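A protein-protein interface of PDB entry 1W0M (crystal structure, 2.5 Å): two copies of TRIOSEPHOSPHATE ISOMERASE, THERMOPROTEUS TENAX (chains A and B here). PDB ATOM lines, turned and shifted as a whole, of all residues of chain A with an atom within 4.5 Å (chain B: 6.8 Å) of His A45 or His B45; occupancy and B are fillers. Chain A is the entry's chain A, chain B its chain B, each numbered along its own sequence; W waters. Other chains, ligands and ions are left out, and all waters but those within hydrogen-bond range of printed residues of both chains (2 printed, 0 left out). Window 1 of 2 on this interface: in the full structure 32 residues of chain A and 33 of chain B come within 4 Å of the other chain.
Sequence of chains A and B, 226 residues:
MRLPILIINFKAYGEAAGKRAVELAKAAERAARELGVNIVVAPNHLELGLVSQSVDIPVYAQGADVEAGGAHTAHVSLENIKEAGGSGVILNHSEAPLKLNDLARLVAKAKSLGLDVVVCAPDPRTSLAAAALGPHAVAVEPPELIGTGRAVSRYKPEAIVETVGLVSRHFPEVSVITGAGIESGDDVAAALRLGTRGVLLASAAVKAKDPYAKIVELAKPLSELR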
ATOM      1  N   PRO A  43       5.748  -8.519  15.112  1.00  0.00           N
ATOM      2  CA  PRO A  43       6.816  -9.407  15.569  1.00  0.00           C
ATOM      3  C   PRO A  43       8.023  -9.368  14.644  1.00  0.00           C
ATOM      4  O   PRO A  43       7.912  -8.839  13.541  1.00  0.00           O
ATOM      5  CB  PRO A  43       6.133 -10.759  15.557  1.00  0.00           C
ATOM      6  CG  PRO A  43       5.266 -10.652  14.364  1.00  0.00           C
ATOM      7  CD  PRO A  43       4.654  -9.284  14.495  1.00  0.00           C
ATOM      8  N   ASN A  44       9.174  -9.897  15.074  1.00  0.00           N
ATOM      9  CA  ASN A  44      10.303  -9.889  14.169  1.00  0.00           C
ATOM     10  C   ASN A  44       9.938 -10.791  12.983  1.00  0.00           C
ATOM     11  O   ASN A  44       9.073 -11.677  13.075  1.00  0.00           O
ATOM     12  CB  ASN A  44      11.628 -10.328  14.843  1.00  0.00           C
ATOM     13  CG  ASN A  44      11.702 -11.824  15.144  1.00  0.00           C
ATOM     14  OD1 ASN A  44      11.406 -12.655  14.285  1.00  0.00           O
ATOM     15  ND2 ASN A  44      12.134 -12.175  16.362  1.00  0.00           N
ATOM     16  N   HIS A  45      10.590 -10.537  11.857  1.00  0.00           N
ATOM     17  CA  HIS A  45      10.350 -11.289  10.637  1.00  0.00           C
ATOM     18  C   HIS A  45      10.208 -12.797  10.810  1.00  0.00           C
ATOM     19  O   HIS A  45       9.257 -13.388  10.300  1.00  0.00           O
ATOM     20  CB  HIS A  45      11.449 -10.964   9.636  1.00  0.00           C
ATOM     21  CG  HIS A  45      11.336  -9.586   9.064  1.00  0.00           C
ATOM     22  ND1 HIS A  45      12.432  -8.854   8.657  1.00  0.00           N
ATOM     23  CD2 HIS A  45      10.250  -8.816   8.805  1.00  0.00           C
ATOM     24  CE1 HIS A  45      12.024  -7.694   8.171  1.00  0.00           C
ATOM     25  NE2 HIS A  45      10.705  -7.647   8.248  1.00  0.00           N
ATOM     26  N   LEU A  46      11.149 -13.400  11.531  1.00  0.00           N
ATOM     27  CA  LEU A  46      11.183 -14.841  11.771  1.00  0.00           C
ATOM     28  C   LEU A  46       9.918 -15.424  12.409  1.00  0.00           C
ATOM     29  O   LEU A  46       9.599 -16.587  12.205  1.00  0.00           O
ATOM     30  CB  LEU A  46      12.382 -15.178  12.653  1.00  0.00           C
ATOM     31  CG  LEU A  46      13.721 -14.604  12.184  1.00  0.00           C
ATOM     32  CD1 LEU A  46      14.793 -14.923  13.223  1.00  0.00           C
ATOM     33  CD2 LEU A  46      14.109 -15.166  10.819  1.00  0.00           C
ATOM     34  N   GLU A  47       9.195 -14.616  13.172  1.00  0.00           N
ATOM     35  CA  GLU A  47       7.974 -15.101  13.825  1.00  0.00           C
ATOM     36  C   GLU A  47       6.689 -14.561  13.201  1.00  0.00           C
ATOM     37  O   GLU A  47       5.604 -14.854  13.707  1.00  0.00           O
ATOM     38  CB  GLU A  47       7.975 -14.695  15.304  1.00  0.00           C
ATOM     39  CG  GLU A  47       9.269 -14.957  16.065  1.00  0.00           C
ATOM     40  CD  GLU A  47       9.626 -16.434  16.103  1.00  0.00           C
ATOM     41  OE1 GLU A  47       8.712 -17.260  15.881  1.00  0.00           O
ATOM     42  OE2 GLU A  47      10.800 -16.780  16.361  1.00  0.00           O
ATOM     43  N   LEU A  48       6.790 -13.776  12.127  1.00  0.00           N
ATOM     44  CA  LEU A  48       5.585 -13.185  11.544  1.00  0.00           C
ATOM     45  C   LEU A  48       4.524 -14.191  11.128  1.00  0.00           C
ATOM     46  O   LEU A  48       3.362 -14.045  11.499  1.00  0.00           O
ATOM     47  CB  LEU A  48       5.915 -12.270  10.352  1.00  0.00           C
ATOM     48  CG  LEU A  48       4.631 -11.561   9.888  1.00  0.00           C
ATOM     49  CD1 LEU A  48       4.792 -10.068   9.955  1.00  0.00           C
ATOM     50  CD2 LEU A  48       4.256 -12.023   8.501  1.00  0.00           C
ATOM     51  N   GLN A  62       7.500  -5.703  10.374  1.00  0.00           N
ATOM     52  CA  GLN A  62       8.345  -4.607  10.843  1.00  0.00           C
ATOM     53  C   GLN A  62       8.978  -3.825   9.689  1.00  0.00           C
ATOM     54  O   GLN A  62       9.526  -2.748   9.890  1.00  0.00           O
ATOM     55  CB  GLN A  62       9.449  -5.163  11.747  1.00  0.00           C
ATOM     56  CG  GLN A  62       8.959  -5.586  13.120  1.00  0.00           C
ATOM     57  CD  GLN A  62      10.076  -6.158  13.992  1.00  0.00           C
ATOM     58  OE1 GLN A  62      11.258  -6.102  13.643  1.00  0.00           O
ATOM     59  NE2 GLN A  62       9.701  -6.697  15.139  1.00  0.00           N
ATOM     60  N   GLY A  63       8.915  -4.395   8.491  1.00  0.00           N
ATOM     61  CA  GLY A  63       9.471  -3.773   7.305  1.00  0.00           C
ATOM     62  C   GLY A  63       9.425  -4.725   6.106  1.00  0.00           C
ATOM     63  O   GLY A  63       8.980  -5.889   6.208  1.00  0.00           O
ATOM     64  N   ALA A  74      16.752 -14.062   1.393  1.00  0.00           N
ATOM     65  CA  ALA A  74      16.924 -13.250   2.597  1.00  0.00           C
ATOM     66  C   ALA A  74      16.196 -11.904   2.572  1.00  0.00           C
ATOM     67  O   ALA A  74      16.454 -11.037   3.402  1.00  0.00           O
ATOM     68  CB  ALA A  74      18.446 -13.048   2.902  1.00  0.00           C
ATOM     69  N   VAL A  76      12.426  -9.638   2.387  1.00  0.00           N
ATOM     70  CA  VAL A  76      11.045  -9.711   2.816  1.00  0.00           C
ATOM     71  C   VAL A  76      10.220  -8.943   1.773  1.00  0.00           C
ATOM     72  O   VAL A  76      10.335  -7.731   1.645  1.00  0.00           O
ATOM     73  CB  VAL A  76      10.852  -9.056   4.210  1.00  0.00           C
ATOM     74  CG1 VAL A  76       9.368  -8.984   4.568  1.00  0.00           C
ATOM     75  CG2 VAL A  76      11.551  -9.869   5.258  1.00  0.00           C
ATOM     76  N   LYS B  11      13.951 -19.178  -1.099  1.00  0.00           N
ATOM     77  CA  LYS B  11      14.031 -17.780  -1.519  1.00  0.00           C
ATOM     78  C   LYS B  11      12.713 -17.086  -1.118  1.00  0.00           C
ATOM     79  O   LYS B  11      12.156 -17.376  -0.045  1.00  0.00           O
ATOM     80  CB  LYS B  11      14.294 -17.686  -3.023  1.00  0.00           C
ATOM     81  CG  LYS B  11      15.589 -18.382  -3.420  1.00  0.00           C
ATOM     82  CD  LYS B  11      16.076 -17.997  -4.806  1.00  0.00           C
ATOM     83  CE  LYS B  11      17.458 -18.580  -5.034  1.00  0.00           C
ATOM     84  NZ  LYS B  11      18.028 -18.236  -6.352  1.00  0.00           N
ATOM     85  N   ALA B  42      15.541 -23.980   3.904  1.00  0.00           N
ATOM     86  CA  ALA B  42      15.708 -22.540   4.211  1.00  0.00           C
ATOM     87  C   ALA B  42      14.505 -21.726   3.725  1.00  0.00           C
ATOM     88  O   ALA B  42      14.504 -21.206   2.613  1.00  0.00           O
ATOM     89  CB  ALA B  42      16.967 -22.004   3.559  1.00  0.00           C
ATOM     90  N   PRO B  43      13.468 -21.601   4.557  1.00  0.00           N
ATOM     91  CA  PRO B  43      12.267 -20.838   4.170  1.00  0.00           C
ATOM     92  C   PRO B  43      12.485 -19.332   4.230  1.00  0.00           C
ATOM     93  O   PRO B  43      13.483 -18.875   4.793  1.00  0.00           O
ATOM     94  CB  PRO B  43      11.228 -21.294   5.190  1.00  0.00           C
ATOM     95  CG  PRO B  43      12.088 -21.478   6.453  1.00  0.00           C
ATOM     96  CD  PRO B  43      13.328 -22.190   5.908  1.00  0.00           C
ATOM     97  N   ASN B  44      11.571 -18.547   3.660  1.00  0.00           N
ATOM     98  CA  ASN B  44      11.760 -17.110   3.750  1.00  0.00           C
ATOM     99  C   ASN B  44      11.634 -16.735   5.244  1.00  0.00           C
ATOM    100  O   ASN B  44      11.029 -17.460   6.045  1.00  0.00           O
ATOM    101  CB  ASN B  44      10.770 -16.330   2.858  1.00  0.00           C
ATOM    102  CG  ASN B  44       9.346 -16.299   3.400  1.00  0.00           C
ATOM    103  OD1 ASN B  44       9.126 -16.079   4.589  1.00  0.00           O
ATOM    104  ND2 ASN B  44       8.361 -16.474   2.509  1.00  0.00           N
ATOM    105  N   HIS B  45      12.241 -15.621   5.617  1.00  0.00           N
ATOM    106  CA  HIS B  45      12.238 -15.170   6.995  1.00  0.00           C
ATOM    107  C   HIS B  45      10.900 -15.233   7.707  1.00  0.00           C
ATOM    108  O   HIS B  45      10.834 -15.623   8.877  1.00  0.00           O
ATOM    109  CB  HIS B  45      12.777 -13.732   7.063  1.00  0.00           C
ATOM    110  CG  HIS B  45      14.239 -13.624   6.744  1.00  0.00           C
ATOM    111  ND1 HIS B  45      14.799 -12.505   6.163  1.00  0.00           N
ATOM    112  CD2 HIS B  45      15.260 -14.487   6.953  1.00  0.00           C
ATOM    113  CE1 HIS B  45      16.102 -12.680   6.028  1.00  0.00           C
ATOM    114  NE2 HIS B  45      16.408 -13.874   6.504  1.00  0.00           N
ATOM    115  N   LEU B  46       9.846 -14.832   7.012  1.00  0.00           N
ATOM    116  CA  LEU B  46       8.519 -14.780   7.595  1.00  0.00           C
ATOM    117  C   LEU B  46       7.996 -16.129   8.065  1.00  0.00           C
ATOM    118  O   LEU B  46       7.160 -16.192   8.992  1.00  0.00           O
ATOM    119  CB  LEU B  46       7.528 -14.179   6.590  1.00  0.00           C
ATOM    120  CG  LEU B  46       7.925 -12.826   6.001  1.00  0.00           C
ATOM    121  CD1 LEU B  46       6.950 -12.434   4.915  1.00  0.00           C
ATOM    122  CD2 LEU B  46       7.982 -11.781   7.102  1.00  0.00           C
ATOM    123  N   GLU B  47       8.490 -17.199   7.440  1.00  0.00           N
ATOM    124  CA  GLU B  47       8.035 -18.531   7.788  1.00  0.00           C
ATOM    125  C   GLU B  47       9.058 -19.325   8.589  1.00  0.00           C
ATOM    126  O   GLU B  47       8.788 -20.469   8.948  1.00  0.00           O
ATOM    127  CB  GLU B  47       7.711 -19.308   6.510  1.00  0.00           C
ATOM    128  CG  GLU B  47       6.861 -18.578   5.489  1.00  0.00           C
ATOM    129  CD  GLU B  47       5.502 -18.192   6.023  1.00  0.00           C
ATOM    130  OE1 GLU B  47       5.069 -18.739   7.075  1.00  0.00           O
ATOM    131  OE2 GLU B  47       4.858 -17.344   5.377  1.00  0.00           O
ATOM    132  N   LEU B  48      10.221 -18.743   8.877  1.00  0.00           N
ATOM    133  CA  LEU B  48      11.244 -19.489   9.589  1.00  0.00           C
ATOM    134  C   LEU B  48      10.783 -20.114  10.913  1.00  0.00           C
ATOM    135  O   LEU B  48      10.954 -21.320  11.109  1.00  0.00           O
ATOM    136  CB  LEU B  48      12.496 -18.642   9.824  1.00  0.00           C
ATOM    137  CG  LEU B  48      13.595 -19.574  10.383  1.00  0.00           C
ATOM    138  CD1 LEU B  48      14.814 -19.601   9.480  1.00  0.00           C
ATOM    139  CD2 LEU B  48      13.965 -19.134  11.792  1.00  0.00           C
ATOM    140  N   GLY B  49      10.210 -19.312  11.813  1.00  0.00           N
ATOM    141  CA  GLY B  49       9.724 -19.844  13.076  1.00  0.00           C
ATOM    142  C   GLY B  49       8.671 -20.928  12.854  1.00  0.00           C
ATOM    143  O   GLY B  49       8.737 -22.023  13.415  1.00  0.00           O
ATOM    144  N   LEU B  50       7.693 -20.628  12.011  1.00  0.00           N
ATOM    145  CA  LEU B  50       6.633 -21.582  11.725  1.00  0.00           C
ATOM    146  C   LEU B  50       7.166 -22.916  11.230  1.00  0.00           C
ATOM    147  O   LEU B  50       6.788 -23.962  11.751  1.00  0.00           O
ATOM    148  CB  LEU B  50       5.673 -21.014  10.685  1.00  0.00           C
ATOM    149  CG  LEU B  50       4.488 -21.904  10.299  1.00  0.00           C
ATOM    150  CD1 LEU B  50       3.619 -22.201  11.514  1.00  0.00           C
ATOM    151  CD2 LEU B  50       3.671 -21.195   9.227  1.00  0.00           C
ATOM    152  N   ALA B  61      18.201 -20.203   8.217  1.00  0.00           N
ATOM    153  CA  ALA B  61      17.712 -18.885   7.851  1.00  0.00           C
ATOM    154  C   ALA B  61      18.416 -18.560   6.533  1.00  0.00           C
ATOM    155  O   ALA B  61      19.558 -18.977   6.314  1.00  0.00           O
ATOM    156  CB  ALA B  61      18.079 -17.865   8.912  1.00  0.00           C
ATOM    157  N   GLN B  62      17.723 -17.831   5.662  1.00  0.00           N
ATOM    158  CA  GLN B  62      18.253 -17.436   4.357  1.00  0.00           C
ATOM    159  C   GLN B  62      19.354 -16.385   4.473  1.00  0.00           C
ATOM    160  O   GLN B  62      20.124 -16.168   3.525  1.00  0.00           O
ATOM    161  CB  GLN B  62      17.122 -16.890   3.474  1.00  0.00           C
ATOM    162  CG  GLN B  62      16.206 -17.986   2.924  1.00  0.00           C
ATOM    163  CD  GLN B  62      15.087 -17.441   2.052  1.00  0.00           C
ATOM    164  OE1 GLN B  62      15.105 -16.271   1.635  1.00  0.00           O
ATOM    165  NE2 GLN B  62      14.107 -18.294   1.755  1.00  0.00           N
ATOM    166  N   GLY B  63      19.403 -15.735   5.642  1.00  0.00           N
ATOM    167  CA  GLY B  63      20.395 -14.720   5.897  1.00  0.00           C
ATOM    168  C   GLY B  63      20.169 -14.087   7.264  1.00  0.00           C
ATOM    169  O   GLY B  63      19.229 -14.455   7.982  1.00  0.00           O
ATOM    170  N   ALA B  64      21.056 -13.161   7.626  1.00  0.00           N
ATOM    171  CA  ALA B  64      20.977 -12.404   8.879  1.00  0.00           C
ATOM    172  C   ALA B  64      21.780 -11.128   8.650  1.00  0.00           C
ATOM    173  O   ALA B  64      22.629 -11.056   7.755  1.00  0.00           O
ATOM    174  CB  ALA B  64      21.573 -13.203  10.057  1.00  0.00           C
ATOM    175  N   THR B  73      14.596  -3.038  14.504  1.00  0.00           N
ATOM    176  CA  THR B  73      13.351  -3.214  13.776  1.00  0.00           C
ATOM    177  C   THR B  73      13.616  -3.639  12.327  1.00  0.00           C
ATOM    178  O   THR B  73      14.463  -3.074  11.641  1.00  0.00           O
ATOM    179  CB  THR B  73      12.510  -1.910  13.763  1.00  0.00           C
ATOM    180  OG1 THR B  73      12.235  -1.471  15.104  1.00  0.00           O
ATOM    181  CG2 THR B  73      11.194  -2.143  13.044  1.00  0.00           C
ATOM    182  N   ALA B  74      12.886  -4.657  11.887  1.00  0.00           N
ATOM    183  CA  ALA B  74      12.983  -5.187  10.538  1.00  0.00           C
ATOM    184  C   ALA B  74      14.298  -5.851  10.212  1.00  0.00           C
ATOM    185  O   ALA B  74      14.602  -6.028   9.041  1.00  0.00           O
ATOM    186  CB  ALA B  74      12.686  -4.091   9.502  1.00  0.00           C
ATOM    187  N   HIS B  75      15.088  -6.217  11.222  1.00  0.00           N
ATOM    188  CA  HIS B  75      16.354  -6.895  10.960  1.00  0.00           C
ATOM    189  C   HIS B  75      16.239  -8.326  11.416  1.00  0.00           C
ATOM    190  O   HIS B  75      15.294  -8.680  12.143  1.00  0.00           O
ATOM    191  CB  HIS B  75      17.504  -6.219  11.694  1.00  0.00           C
ATOM    192  CG  HIS B  75      17.792  -4.847  11.187  1.00  0.00           C
ATOM    193  ND1 HIS B  75      18.452  -4.626   9.997  1.00  0.00           N
ATOM    194  CD2 HIS B  75      17.404  -3.627  11.634  1.00  0.00           C
ATOM    195  CE1 HIS B  75      18.457  -3.329   9.734  1.00  0.00           C
ATOM    196  NE2 HIS B  75      17.826  -2.702  10.710  1.00  0.00           N
ATOM    197  N   VAL B  76      17.178  -9.162  10.964  1.00  0.00           N
ATOM    198  CA  VAL B  76      17.188 -10.563  11.359  1.00  0.00           C
ATOM    199  C   VAL B  76      18.470 -10.802  12.137  1.00  0.00           C
ATOM    200  O   VAL B  76      19.585 -10.655  11.594  1.00  0.00           O
ATOM    201  CB  VAL B  76      17.108 -11.506  10.127  1.00  0.00           C
ATOM    202  CG1 VAL B  76      17.303 -12.967  10.563  1.00  0.00           C
ATOM    203  CG2 VAL B  76      15.732 -11.364   9.464  1.00  0.00           C
ATOM    204  N   ILE B  81      17.332 -16.027  15.321  1.00  0.00           N
ATOM    205  CA  ILE B  81      17.221 -17.200  14.474  1.00  0.00           C
ATOM    206  C   ILE B  81      17.270 -18.428  15.373  1.00  0.00           C
ATOM    207  O   ILE B  81      16.466 -19.350  15.233  1.00  0.00           O
ATOM    208  CB  ILE B  81      18.375 -17.262  13.435  1.00  0.00           C
ATOM    209  CG1 ILE B  81      18.167 -16.188  12.368  1.00  0.00           C
ATOM    210  CG2 ILE B  81      18.430 -18.660  12.766  1.00  0.00           C
ATOM    211  CD1 ILE B  81      19.363 -16.021  11.423  1.00  0.00           C
HETATM  212  O   HOH W   1       7.210 -17.638  11.345  1.00  0.00           O
HETATM  213  O   HOH W   2      12.611  -8.449  12.226  1.00  0.00           O
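Water W2 lies within hydrogen-bond range of O of His B75 (2.7 Å), N of His A45 (2.9 Å) and OE1 of Gln A62 (3.1 Å).
Water W1 lies within hydrogen-bond range of the backbone carbonyl oxygen (O) of Leu A46 (2.7 Å), the backbone carbonyl oxygen (O) of Leu B46 (2.8 Å), the backbone NH (N) of Leu B50 (3.1 Å) and the backbone NH (N) of Gly B49 (3.5 Å).
His A45 touches Leu B46, and with the chains exchanged Leu A46 touches His B45.
Leu A46 touches Val B76, but with the chains exchanged Val A76 does not touch Leu B46 (4.02 Å).
Gln A62 touches Ala B74, and with the chains exchanged Ala A74 touches Gln B62.
Gly A63 touches Ala B74, and with the chains exchanged Ala A74 touches Gly B63.
Of the 16 pairs that touch across the chains among the printed residues, 11 have their exchanged pair printed and touching as well.
The side-chain amide nitrogen (NE2) of Gln B62 lies within hydrogen-bond range of the backbone carbonyl oxygen (O) of Lys B11 (2.8 Å).
OD1 of Asn A44 is in hydrogen-bond range of N of Glu A47, 3.2 Å away.
A ring nitrogen (NE2) of His A45 is in hydrogen-bond range of the backbone carbonyl oxygen of Gly A63 (3.2 Å).
The backbone NH of Asn A44 lies close to the side-chain amide nitrogen of Gln A62.
The backbone NH of Leu B46 sits at hydrogen-bond distance from the side-chain amide oxygen of Asn B44, 2.8 Å away.
The backbone NH (N) of Asn B44 sits close to the side-chain amide nitrogen (NE2) of Gln B62 (3.2 Å).
His A45 touches just these residues of chain B: His B45 (3.1 Å), Leu B46 (3.1 Å) and Ala B74 (3.2 Å).
Printed residues of chain B within 4 Å of Gln A62: Thr B73 (3.6 Å) and Ala B74 (2.8 Å).
Of chain A, only His A45 (3.1 Å), Leu A46 (3.0 Å) and Ala A74 (3.1 Å) come within 4 Å of His B45.
Of the printed residues of chain A, Leu B46 touches His A45 and Leu A48.
Printed residues of chain A within 4 Å of Thr B73: Gln A62 (3.6 Å).
The nearest residue of chain A that does not touch His B45 is Val A76 (4.3 Å).
Printed residues of chain B that touch a printed residue of chain A: His B45, Leu B46, Leu B48, Gly B49, Gln B62, Gly B63, Thr B73, Ala B74, Val B76 and Ile B81.
Hydrophobic or aromatic side chains of chain B that line the printed part of chain A: His B45, Leu B46, Leu B48, Ala B74, Val B76 and Ile B81.
Along chain B the printed residues that touch a printed residue of chain A span positions 45 to 81.
Of the 10 printed residues of chain A, 7 touch a printed residue of chain B.
Among the printed residues, 16 pairs touch across the chains.
Among the printed residues, no Asp or Glu carboxylate lies within 4 Å of a Lys or Arg side-chain nitrogen of the other chain.
The backbone carbonyl oxygen of His B45 sits close to the backbone NH of Leu A46, 3.5 Å away.
The backbone carbonyl oxygen (O) of His A45 sits close to the backbone carbonyl oxygen (O) of His B45 (3.1 Å).
The backbone NH of Ala B74 lies within hydrogen-bond range of the side-chain amide oxygen of Gln A62 (2.8 Å).
O of Leu A46 sits at hydrogen-bond distance from N of Gly B49 (2.8 Å).
The backbone NH of Ala A74 is in hydrogen-bond range of the side-chain amide oxygen of Gln B62, 2.8 Å away.
Among the printed residues, merely in contact across the chains: Ala A74 with His B45 (3.1 Å), His A45 with Leu B46 (3.1 Å), His A45 with Ala B74 (3.2 Å), Leu A46 with Ile B81 (3.5 Å), Gln A62 with Thr B73 (3.6 Å), Leu A48 with Leu B46 (3.9 Å), Leu A46 with Val B76 (3.9 Å), Gly A63 with Ala B74 (3.9 Å), Leu A46 with Leu B48 (3.9 Å), Ala A74 with Gly B63 (3.9 Å) and Glu A47 with Gly B49 (3.9 Å).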
